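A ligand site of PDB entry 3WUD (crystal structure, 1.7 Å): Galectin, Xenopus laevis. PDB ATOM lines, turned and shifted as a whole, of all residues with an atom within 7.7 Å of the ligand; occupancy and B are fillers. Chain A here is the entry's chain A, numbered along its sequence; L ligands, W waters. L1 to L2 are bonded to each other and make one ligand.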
ATOM      1  N   SER A  32      10.894 -13.977  10.148  1.00  0.00           N
ATOM      2  CA  SER A  32      11.457 -13.482   8.881  1.00  0.00           C
ATOM      3  C   SER A  32      12.194 -14.664   8.176  1.00  0.00           C
ATOM      4  O   SER A  32      12.407 -15.730   8.790  1.00  0.00           O
ATOM      5  CB  SER A  32      12.480 -12.341   9.133  1.00  0.00           C
ATOM      6  OG  SER A  32      13.542 -12.822   9.877  1.00  0.00           O
ATOM      7  N   PHE A  33      12.544 -14.509   6.952  1.00  0.00           N
ATOM      8  CA  PHE A  33      13.475 -15.443   6.299  1.00  0.00           C
ATOM      9  C   PHE A  33      14.362 -14.619   5.311  1.00  0.00           C
ATOM     10  O   PHE A  33      14.026 -13.462   4.995  1.00  0.00           O
ATOM     11  CB  PHE A  33      12.722 -16.586   5.585  1.00  0.00           C
ATOM     12  CG  PHE A  33      11.880 -16.159   4.397  1.00  0.00           C
ATOM     13  CD1 PHE A  33      12.374 -16.252   3.098  1.00  0.00           C
ATOM     14  CD2 PHE A  33      10.549 -15.738   4.550  1.00  0.00           C
ATOM     15  CE1 PHE A  33      11.627 -15.879   2.005  1.00  0.00           C
ATOM     16  CE2 PHE A  33       9.771 -15.395   3.459  1.00  0.00           C
ATOM     17  CZ  PHE A  33      10.310 -15.457   2.194  1.00  0.00           C
ATOM     18  N   ALA A  34      15.513 -15.168   4.894  1.00  0.00           N
ATOM     19  CA  ALA A  34      16.395 -14.370   4.034  1.00  0.00           C
ATOM     20  C   ALA A  34      16.931 -15.308   2.983  1.00  0.00           C
ATOM     21  O   ALA A  34      17.224 -16.489   3.299  1.00  0.00           O
ATOM     22  CB  ALA A  34      17.537 -13.716   4.834  1.00  0.00           C
ATOM     23  N   ASN A  36      20.083 -14.935   0.245  1.00  0.00           N
ATOM     24  CA  ASN A  36      21.235 -14.195  -0.189  1.00  0.00           C
ATOM     25  C   ASN A  36      21.838 -14.714  -1.493  1.00  0.00           C
ATOM     26  O   ASN A  36      22.021 -15.898  -1.608  1.00  0.00           O
ATOM     27  CB  ASN A  36      22.243 -14.355   0.900  1.00  0.00           C
ATOM     28  CG  ASN A  36      21.766 -13.815   2.225  1.00  0.00           C
ATOM     29  OD1 ASN A  36      21.278 -12.682   2.307  1.00  0.00           O
ATOM     30  ND2 ASN A  36      21.907 -14.607   3.248  1.00  0.00           N
ATOM     31  N   HIS A  47      20.599  -9.358  -0.382  1.00  0.00           N
ATOM     32  CA  HIS A  47      20.078  -9.937   0.806  1.00  0.00           C
ATOM     33  C   HIS A  47      18.617  -9.570   0.727  1.00  0.00           C
ATOM     34  O   HIS A  47      18.275  -8.365   0.785  1.00  0.00           O
ATOM     35  CB  HIS A  47      20.749  -9.343   2.045  1.00  0.00           C
ATOM     36  CG  HIS A  47      20.074  -9.671   3.361  1.00  0.00           C
ATOM     37  ND1 HIS A  47      20.171 -10.897   3.980  1.00  0.00           N
ATOM     38  CD2 HIS A  47      19.365  -8.877   4.180  1.00  0.00           C
ATOM     39  CE1 HIS A  47      19.546 -10.830   5.153  1.00  0.00           C
ATOM     40  NE2 HIS A  47      19.109  -9.598   5.315  1.00  0.00           N
ATOM     41  N   PHE A  48      17.781 -10.577   0.537  1.00  0.00           N
ATOM     42  CA  PHE A  48      16.355 -10.479   0.315  1.00  0.00           C
ATOM     43  C   PHE A  48      15.653 -11.003   1.562  1.00  0.00           C
ATOM     44  O   PHE A  48      15.762 -12.189   1.886  1.00  0.00           O
ATOM     45  CB  PHE A  48      15.987 -11.353  -0.882  1.00  0.00           C
ATOM     46  CG  PHE A  48      14.525 -11.421  -1.165  1.00  0.00           C
ATOM     47  CD1 PHE A  48      13.900 -10.407  -1.891  1.00  0.00           C
ATOM     48  CD2 PHE A  48      13.768 -12.497  -0.721  1.00  0.00           C
ATOM     49  CE1 PHE A  48      12.556 -10.473  -2.173  1.00  0.00           C
ATOM     50  CE2 PHE A  48      12.385 -12.576  -0.976  1.00  0.00           C
ATOM     51  CZ  PHE A  48      11.792 -11.527  -1.686  1.00  0.00           C
ATOM     52  N   ASN A  49      15.096 -10.104   2.374  1.00  0.00           N
ATOM     53  CA  ASN A  49      14.644 -10.426   3.716  1.00  0.00           C
ATOM     54  C   ASN A  49      13.151 -10.008   4.070  1.00  0.00           C
ATOM     55  O   ASN A  49      12.944  -8.949   4.639  1.00  0.00           O
ATOM     56  CB  ASN A  49      15.614  -9.732   4.679  1.00  0.00           C
ATOM     57  CG  ASN A  49      15.404 -10.088   6.160  1.00  0.00           C
ATOM     58  OD1 ASN A  49      15.718  -9.270   7.004  1.00  0.00           O
ATOM     59  ND2 ASN A  49      14.923 -11.277   6.469  1.00  0.00           N
ATOM     60  N   ARG A  51      10.086  -9.850   6.186  1.00  0.00           N
ATOM     61  CA  ARG A  51       9.968  -9.749   7.571  1.00  0.00           C
ATOM     62  C   ARG A  51       8.467  -9.704   7.938  1.00  0.00           C
ATOM     63  O   ARG A  51       7.760  -8.720   7.580  1.00  0.00           O
ATOM     64  CB  ARG A  51      10.596  -8.452   8.077  1.00  0.00           C
ATOM     65  CG  ARG A  51      12.097  -8.415   7.836  1.00  0.00           C
ATOM     66  CD  ARG A  51      12.767  -7.196   8.450  1.00  0.00           C
ATOM     67  NE  ARG A  51      14.235  -7.244   8.232  1.00  0.00           N
ATOM     68  CZ  ARG A  51      15.053  -6.216   8.501  1.00  0.00           C
ATOM     69  NH1 ARG A  51      14.577  -5.116   9.048  1.00  0.00           N
ATOM     70  NH2 ARG A  51      16.360  -6.315   8.305  1.00  0.00           N
ATOM     71  N   HIS A  54      10.057  -8.409  12.452  1.00  0.00           N
ATOM     72  CA  HIS A  54      11.472  -8.491  12.725  1.00  0.00           C
ATOM     73  C   HIS A  54      12.082  -7.142  12.598  1.00  0.00           C
ATOM     74  O   HIS A  54      11.758  -6.386  11.724  1.00  0.00           O
ATOM     75  CB  HIS A  54      12.111  -9.546  11.775  1.00  0.00           C
ATOM     76  CG  HIS A  54      13.579  -9.690  11.964  1.00  0.00           C
ATOM     77  ND1 HIS A  54      14.152 -10.088  13.150  1.00  0.00           N
ATOM     78  CD2 HIS A  54      14.595  -9.514  11.084  1.00  0.00           C
ATOM     79  CE1 HIS A  54      15.472 -10.087  13.016  1.00  0.00           C
ATOM     80  NE2 HIS A  54      15.762  -9.782  11.765  1.00  0.00           N
ATOM     81  N   GLU A  55      12.932  -6.800  13.539  1.00  0.00           N
ATOM     82  CA  GLU A  55      13.579  -5.469  13.568  1.00  0.00           C
ATOM     83  C   GLU A  55      12.579  -4.328  13.472  1.00  0.00           C
ATOM     84  O   GLU A  55      12.900  -3.342  12.872  1.00  0.00           O
ATOM     85  CB  GLU A  55      14.653  -5.333  12.457  1.00  0.00           C
ATOM     86  CG  GLU A  55      15.731  -6.402  12.484  1.00  0.00           C
ATOM     87  CD  GLU A  55      16.828  -6.155  13.516  1.00  0.00           C
ATOM     88  OE1 GLU A  55      17.822  -6.930  13.530  1.00  0.00           O
ATOM     89  OE2 GLU A  55      16.738  -5.175  14.267  1.00  0.00           O
ATOM     90  N   GLY A  56      11.387  -4.462  14.068  1.00  0.00           N
ATOM     91  CA  GLY A  56      10.297  -3.455  13.983  1.00  0.00           C
ATOM     92  C   GLY A  56       9.508  -3.342  12.677  1.00  0.00           C
ATOM     93  O   GLY A  56       8.591  -2.457  12.528  1.00  0.00           O
ATOM     94  N   ASP A  57       9.793  -4.250  11.730  1.00  0.00           N
ATOM     95  CA  ASP A  57       9.162  -4.249  10.416  1.00  0.00           C
ATOM     96  C   ASP A  57       8.100  -5.375  10.410  1.00  0.00           C
ATOM     97  O   ASP A  57       8.405  -6.474  10.927  1.00  0.00           O
ATOM     98  CB  ASP A  57      10.182  -4.500   9.300  1.00  0.00           C
ATOM     99  CG  ASP A  57      11.165  -3.387   9.188  1.00  0.00           C
ATOM    100  OD1 ASP A  57      10.759  -2.217   9.243  1.00  0.00           O
ATOM    101  OD2 ASP A  57      12.355  -3.717   9.116  1.00  0.00           O
ATOM    102  N   ILE A  62      12.760  -6.262   3.313  1.00  0.00           N
ATOM    103  CA  ILE A  62      13.939  -5.372   3.397  1.00  0.00           C
ATOM    104  C   ILE A  62      14.961  -6.019   2.473  1.00  0.00           C
ATOM    105  O   ILE A  62      15.150  -7.232   2.546  1.00  0.00           O
ATOM    106  CB  ILE A  62      14.473  -5.383   4.809  1.00  0.00           C
ATOM    107  CG1 ILE A  62      13.636  -4.469   5.699  1.00  0.00           C
ATOM    108  CG2 ILE A  62      15.932  -4.878   4.851  1.00  0.00           C
ATOM    109  CD1 ILE A  62      12.133  -4.522   5.549  1.00  0.00           C
ATOM    110  N   CYS A  63      15.527  -5.269   1.522  1.00  0.00           N
ATOM    111  CA  CYS A  63      16.671  -5.779   0.745  1.00  0.00           C
ATOM    112  C   CYS A  63      17.903  -4.928   1.057  1.00  0.00           C
ATOM    113  O   CYS A  63      17.826  -3.716   1.357  1.00  0.00           O
ATOM    114  CB  CYS A  63      16.385  -5.667  -0.731  1.00  0.00           C
ATOM    115  SG  CYS A  63      15.045  -6.828  -1.233  1.00  0.00           S
ATOM    116  N   ASN A  64      19.062  -5.551   0.972  1.00  0.00           N
ATOM    117  CA  ASN A  64      20.299  -4.831   1.091  1.00  0.00           C
ATOM    118  C   ASN A  64      21.408  -5.582   0.385  1.00  0.00           C
ATOM    119  O   ASN A  64      21.230  -6.688  -0.056  1.00  0.00           O
ATOM    120  CB  ASN A  64      20.660  -4.703   2.584  1.00  0.00           C
ATOM    121  CG  ASN A  64      21.521  -3.452   2.867  1.00  0.00           C
ATOM    122  OD1 ASN A  64      22.133  -2.904   2.018  1.00  0.00           O
ATOM    123  ND2 ASN A  64      21.641  -3.088   4.099  1.00  0.00           N
ATOM    124  N   SER A  65      22.526  -4.945   0.225  1.00  0.00           N
ATOM    125  CA  SER A  65      23.744  -5.559  -0.259  1.00  0.00           C
ATOM    126  C   SER A  65      24.695  -5.765   0.877  1.00  0.00           C
ATOM    127  O   SER A  65      24.612  -5.063   1.910  1.00  0.00           O
ATOM    128  CB  SER A  65      24.412  -4.640  -1.310  1.00  0.00           C
ATOM    129  OG  SER A  65      24.731  -3.335  -0.830  1.00  0.00           O
ATOM    130  N   TRP A  71      27.133  -4.167   5.475  1.00  0.00           N
ATOM    131  CA  TRP A  71      25.839  -3.824   4.895  1.00  0.00           C
ATOM    132  C   TRP A  71      25.861  -2.488   4.092  1.00  0.00           C
ATOM    133  O   TRP A  71      26.429  -1.468   4.530  1.00  0.00           O
ATOM    134  CB  TRP A  71      24.709  -3.775   5.942  1.00  0.00           C
ATOM    135  CG  TRP A  71      24.423  -5.072   6.600  1.00  0.00           C
ATOM    136  CD1 TRP A  71      24.611  -5.401   7.957  1.00  0.00           C
ATOM    137  CD2 TRP A  71      23.972  -6.263   5.973  1.00  0.00           C
ATOM    138  NE1 TRP A  71      24.266  -6.698   8.140  1.00  0.00           N
ATOM    139  CE2 TRP A  71      23.803  -7.227   6.970  1.00  0.00           C
ATOM    140  CE3 TRP A  71      23.517  -6.545   4.696  1.00  0.00           C
ATOM    141  CZ2 TRP A  71      23.350  -8.527   6.681  1.00  0.00           C
ATOM    142  CZ3 TRP A  71      23.046  -7.814   4.426  1.00  0.00           C
ATOM    143  CH2 TRP A  71      22.961  -8.776   5.366  1.00  0.00           C
ATOM    144  N   GLY A  72      25.179  -2.459   2.945  1.00  0.00           N
ATOM    145  CA  GLY A  72      24.893  -1.228   2.243  1.00  0.00           C
ATOM    146  C   GLY A  72      23.667  -0.486   2.720  1.00  0.00           C
ATOM    147  O   GLY A  72      23.266  -0.593   3.877  1.00  0.00           O
ATOM    148  N   THR A  73      23.092   0.287   1.839  1.00  0.00           N
ATOM    149  CA  THR A  73      21.844   1.021   2.088  1.00  0.00           C
ATOM    150  C   THR A  73      20.595   0.122   1.909  1.00  0.00           C
ATOM    151  O   THR A  73      20.420  -0.438   0.805  1.00  0.00           O
ATOM    152  CB  THR A  73      21.757   2.227   1.137  1.00  0.00           C
ATOM    153  OG1 THR A  73      22.894   3.070   1.413  1.00  0.00           O
ATOM    154  CG2 THR A  73      20.472   3.064   1.374  1.00  0.00           C
ATOM    155  N   GLU A  74      19.709   0.020   2.942  1.00  0.00           N
ATOM    156  CA  GLU A  74      18.539  -0.813   2.771  1.00  0.00           C
ATOM    157  C   GLU A  74      17.545  -0.254   1.763  1.00  0.00           C
ATOM    158  O   GLU A  74      17.384   0.967   1.682  1.00  0.00           O
ATOM    159  CB  GLU A  74      17.778  -0.945   4.087  1.00  0.00           C
ATOM    160  CG  GLU A  74      18.420  -1.838   5.106  1.00  0.00           C
ATOM    161  CD  GLU A  74      17.662  -1.930   6.444  1.00  0.00           C
ATOM    162  OE1 GLU A  74      16.627  -1.297   6.653  1.00  0.00           O
ATOM    163  OE2 GLU A  74      18.087  -2.711   7.261  1.00  0.00           O
ATOM    164  N   GLN A  75      16.877  -1.170   1.073  1.00  0.00           N
ATOM    165  CA  GLN A  75      15.722  -0.864   0.208  1.00  0.00           C
ATOM    166  C   GLN A  75      14.488  -1.572   0.839  1.00  0.00           C
ATOM    167  O   GLN A  75      14.515  -2.768   1.143  1.00  0.00           O
ATOM    168  CB  GLN A  75      16.003  -1.303  -1.235  1.00  0.00           C
ATOM    169  CG  GLN A  75      14.948  -0.837  -2.212  1.00  0.00           C
ATOM    170  CD  GLN A  75      15.268  -1.254  -3.631  1.00  0.00           C
ATOM    171  OE1 GLN A  75      16.290  -0.817  -4.203  1.00  0.00           O
ATOM    172  NE2 GLN A  75      14.428  -2.089  -4.207  1.00  0.00           N
ATOM    173  N   ARG A  76      13.450  -0.788   1.118  1.00  0.00           N
ATOM    174  CA  ARG A  76      12.248  -1.316   1.737  1.00  0.00           C
ATOM    175  C   ARG A  76      11.080  -1.415   0.714  1.00  0.00           C
ATOM    176  O   ARG A  76      10.730  -0.432   0.021  1.00  0.00           O
ATOM    177  CB  ARG A  76      11.853  -0.518   2.986  1.00  0.00           C
ATOM    178  CG  ARG A  76      12.176  -1.172   4.324  1.00  0.00           C
ATOM    179  CD  ARG A  76      11.864  -0.316   5.577  1.00  0.00           C
ATOM    180  NE  ARG A  76      12.476  -0.906   6.798  1.00  0.00           N
ATOM    181  CZ  ARG A  76      13.784  -0.829   7.114  1.00  0.00           C
ATOM    182  NH1 ARG A  76      14.606  -0.114   6.337  1.00  0.00           N
ATOM    183  NH2 ARG A  76      14.265  -1.424   8.241  1.00  0.00           N
ATOM    184  N   ASP A 126      18.048 -18.686   4.980  1.00  0.00           N
ATOM    185  CA  ASP A 126      17.878 -18.884   6.406  1.00  0.00           C
ATOM    186  C   ASP A 126      16.380 -18.615   6.700  1.00  0.00           C
ATOM    187  O   ASP A 126      15.787 -17.727   6.133  1.00  0.00           O
ATOM    188  CB  ASP A 126      18.784 -17.907   7.175  1.00  0.00           C
ATOM    189  CG  ASP A 126      18.822 -18.153   8.686  1.00  0.00           C
ATOM    190  OD1 ASP A 126      18.623 -19.301   9.218  1.00  0.00           O
ATOM    191  OD2 ASP A 126      19.083 -17.139   9.365  1.00  0.00           O
HETATM  192  C1  LIG L   1      18.430  -0.972  11.486  1.00  0.00           C
HETATM  193  C2  LIG L   1      17.335  -1.643  10.694  1.00  0.00           C
HETATM  194  C3  LIG L   1      17.429  -3.132  10.529  1.00  0.00           C
HETATM  195  C4  LIG L   1      18.853  -3.696  10.688  1.00  0.00           C
HETATM  196  C5  LIG L   1      19.591  -3.143  11.909  1.00  0.00           C
HETATM  197  C6  LIG L   1      21.059  -3.400  11.849  1.00  0.00           C
HETATM  198  O1  LIG L   1      17.997   0.129  12.250  1.00  0.00           O
HETATM  199  O2  LIG L   1      16.011  -1.244  10.957  1.00  0.00           O
HETATM  200  O3  LIG L   1      16.826  -3.409   9.256  1.00  0.00           O
HETATM  201  O4  LIG L   1      18.667  -5.057  10.849  1.00  0.00           O
HETATM  202  O5  LIG L   1      19.474  -1.758  12.030  1.00  0.00           O
HETATM  203  O6  LIG L   1      21.578  -2.879  13.066  1.00  0.00           O
HETATM  204  C1  LG2 L   2      19.554  -5.801   9.961  1.00  0.00           C
HETATM  205  C2  LG2 L   2      19.445  -7.299  10.251  1.00  0.00           C
HETATM  206  C3  LG2 L   2      20.276  -8.167   9.300  1.00  0.00           C
HETATM  207  C4  LG2 L   2      19.986  -7.717   7.860  1.00  0.00           C
HETATM  208  C5  LG2 L   2      20.144  -6.196   7.751  1.00  0.00           C
HETATM  209  C6  LG2 L   2      19.873  -5.618   6.374  1.00  0.00           C
HETATM  210  O1  LG2 L   2      19.912  -7.558  11.561  1.00  0.00           O
HETATM  211  O2  LG2 L   2      20.009  -9.535   9.571  1.00  0.00           O
HETATM  212  O3  LG2 L   2      18.642  -8.087   7.500  1.00  0.00           O
HETATM  213  O4  LG2 L   2      19.261  -5.477   8.621  1.00  0.00           O
HETATM  214  O5  LG2 L   2      20.044  -4.213   6.299  1.00  0.00           O
HETATM  215  O   HOH W   1      17.356 -10.354   9.067  1.00  0.00           O
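The guanidinium group (NH2) of Arg 76 lies within salt-bridge range of the side-chain carboxylate (OE1) of Glu 74 (2.8 Å). The backbone NH of His 47 is in hydrogen-bond range of the backbone carbonyl oxygen of Asn 64, 2.8 Å away. The guanidinium group (NE) of Arg 51 lies within hydrogen-bond range of the side-chain amide oxygen (OD1) of Asn 49 (2.8 Å). The side-chain amide nitrogen (ND2) of Asn 64 is in hydrogen-bond range of the backbone carbonyl oxygen (O) of Gly 72, at 3.0 Å. The side-chain amide oxygen of Asn 64 lies close to the backbone carbonyl oxygen of Thr 73 (3.2 Å). O of Ile 62 is in hydrogen-bond range of N of Asn 49, 2.9 Å away. The backbone carbonyl oxygen of Phe 33 sits at hydrogen-bond distance from the side-chain amide nitrogen of Asn 49, at 2.8 Å. The guanidinium group (NH2) of Arg 76 is in salt-bridge range of the side-chain carboxylate (OD2) of Asp 57 (3.1 Å).
Merely in contact with the ligand: Trp 71. Hydrophobic or aromatic side chains that line the ligand: His 47 and Trp 71. Along chain A the residues within 4 Å of the ligand span positions 47 to 76. The nearest printed residue that does not touch the ligand is Ile 62 (4.3 Å).
Water W1 lies within hydrogen-bond range of an oxygen (O2) of LG2 L2 (2.8 Å), the side-chain amide oxygen of Asn 49 (2.8 Å) and a ring nitrogen (NE2) of His 54 (3.2 Å).
OE2 of Glu 74 lies within hydrogen-bond range of O3 of LIG L1. A ring nitrogen (NE2) of His 47 lies within hydrogen-bond range of an oxygen (O3) of LG2 L2 (2.7 Å). The guanidinium group of Arg 51 sits at hydrogen-bond distance from an oxygen (O3) of LIG L1 (2.8 Å). O1 of LG2 L2 is in hydrogen-bond range of OE1 of Glu 55. An oxygen (O5) of LG2 L2 lies within hydrogen-bond range of the side-chain amide nitrogen (ND2) of Asn 64, at 2.9 Å. An oxygen (O3) of LG2 L2 lies within hydrogen-bond range of the side-chain amide oxygen of Asn 49. An oxygen (O2) of LIG L1 lies within hydrogen-bond range of the guanidinium group of Arg 76, at 3.2 Å.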
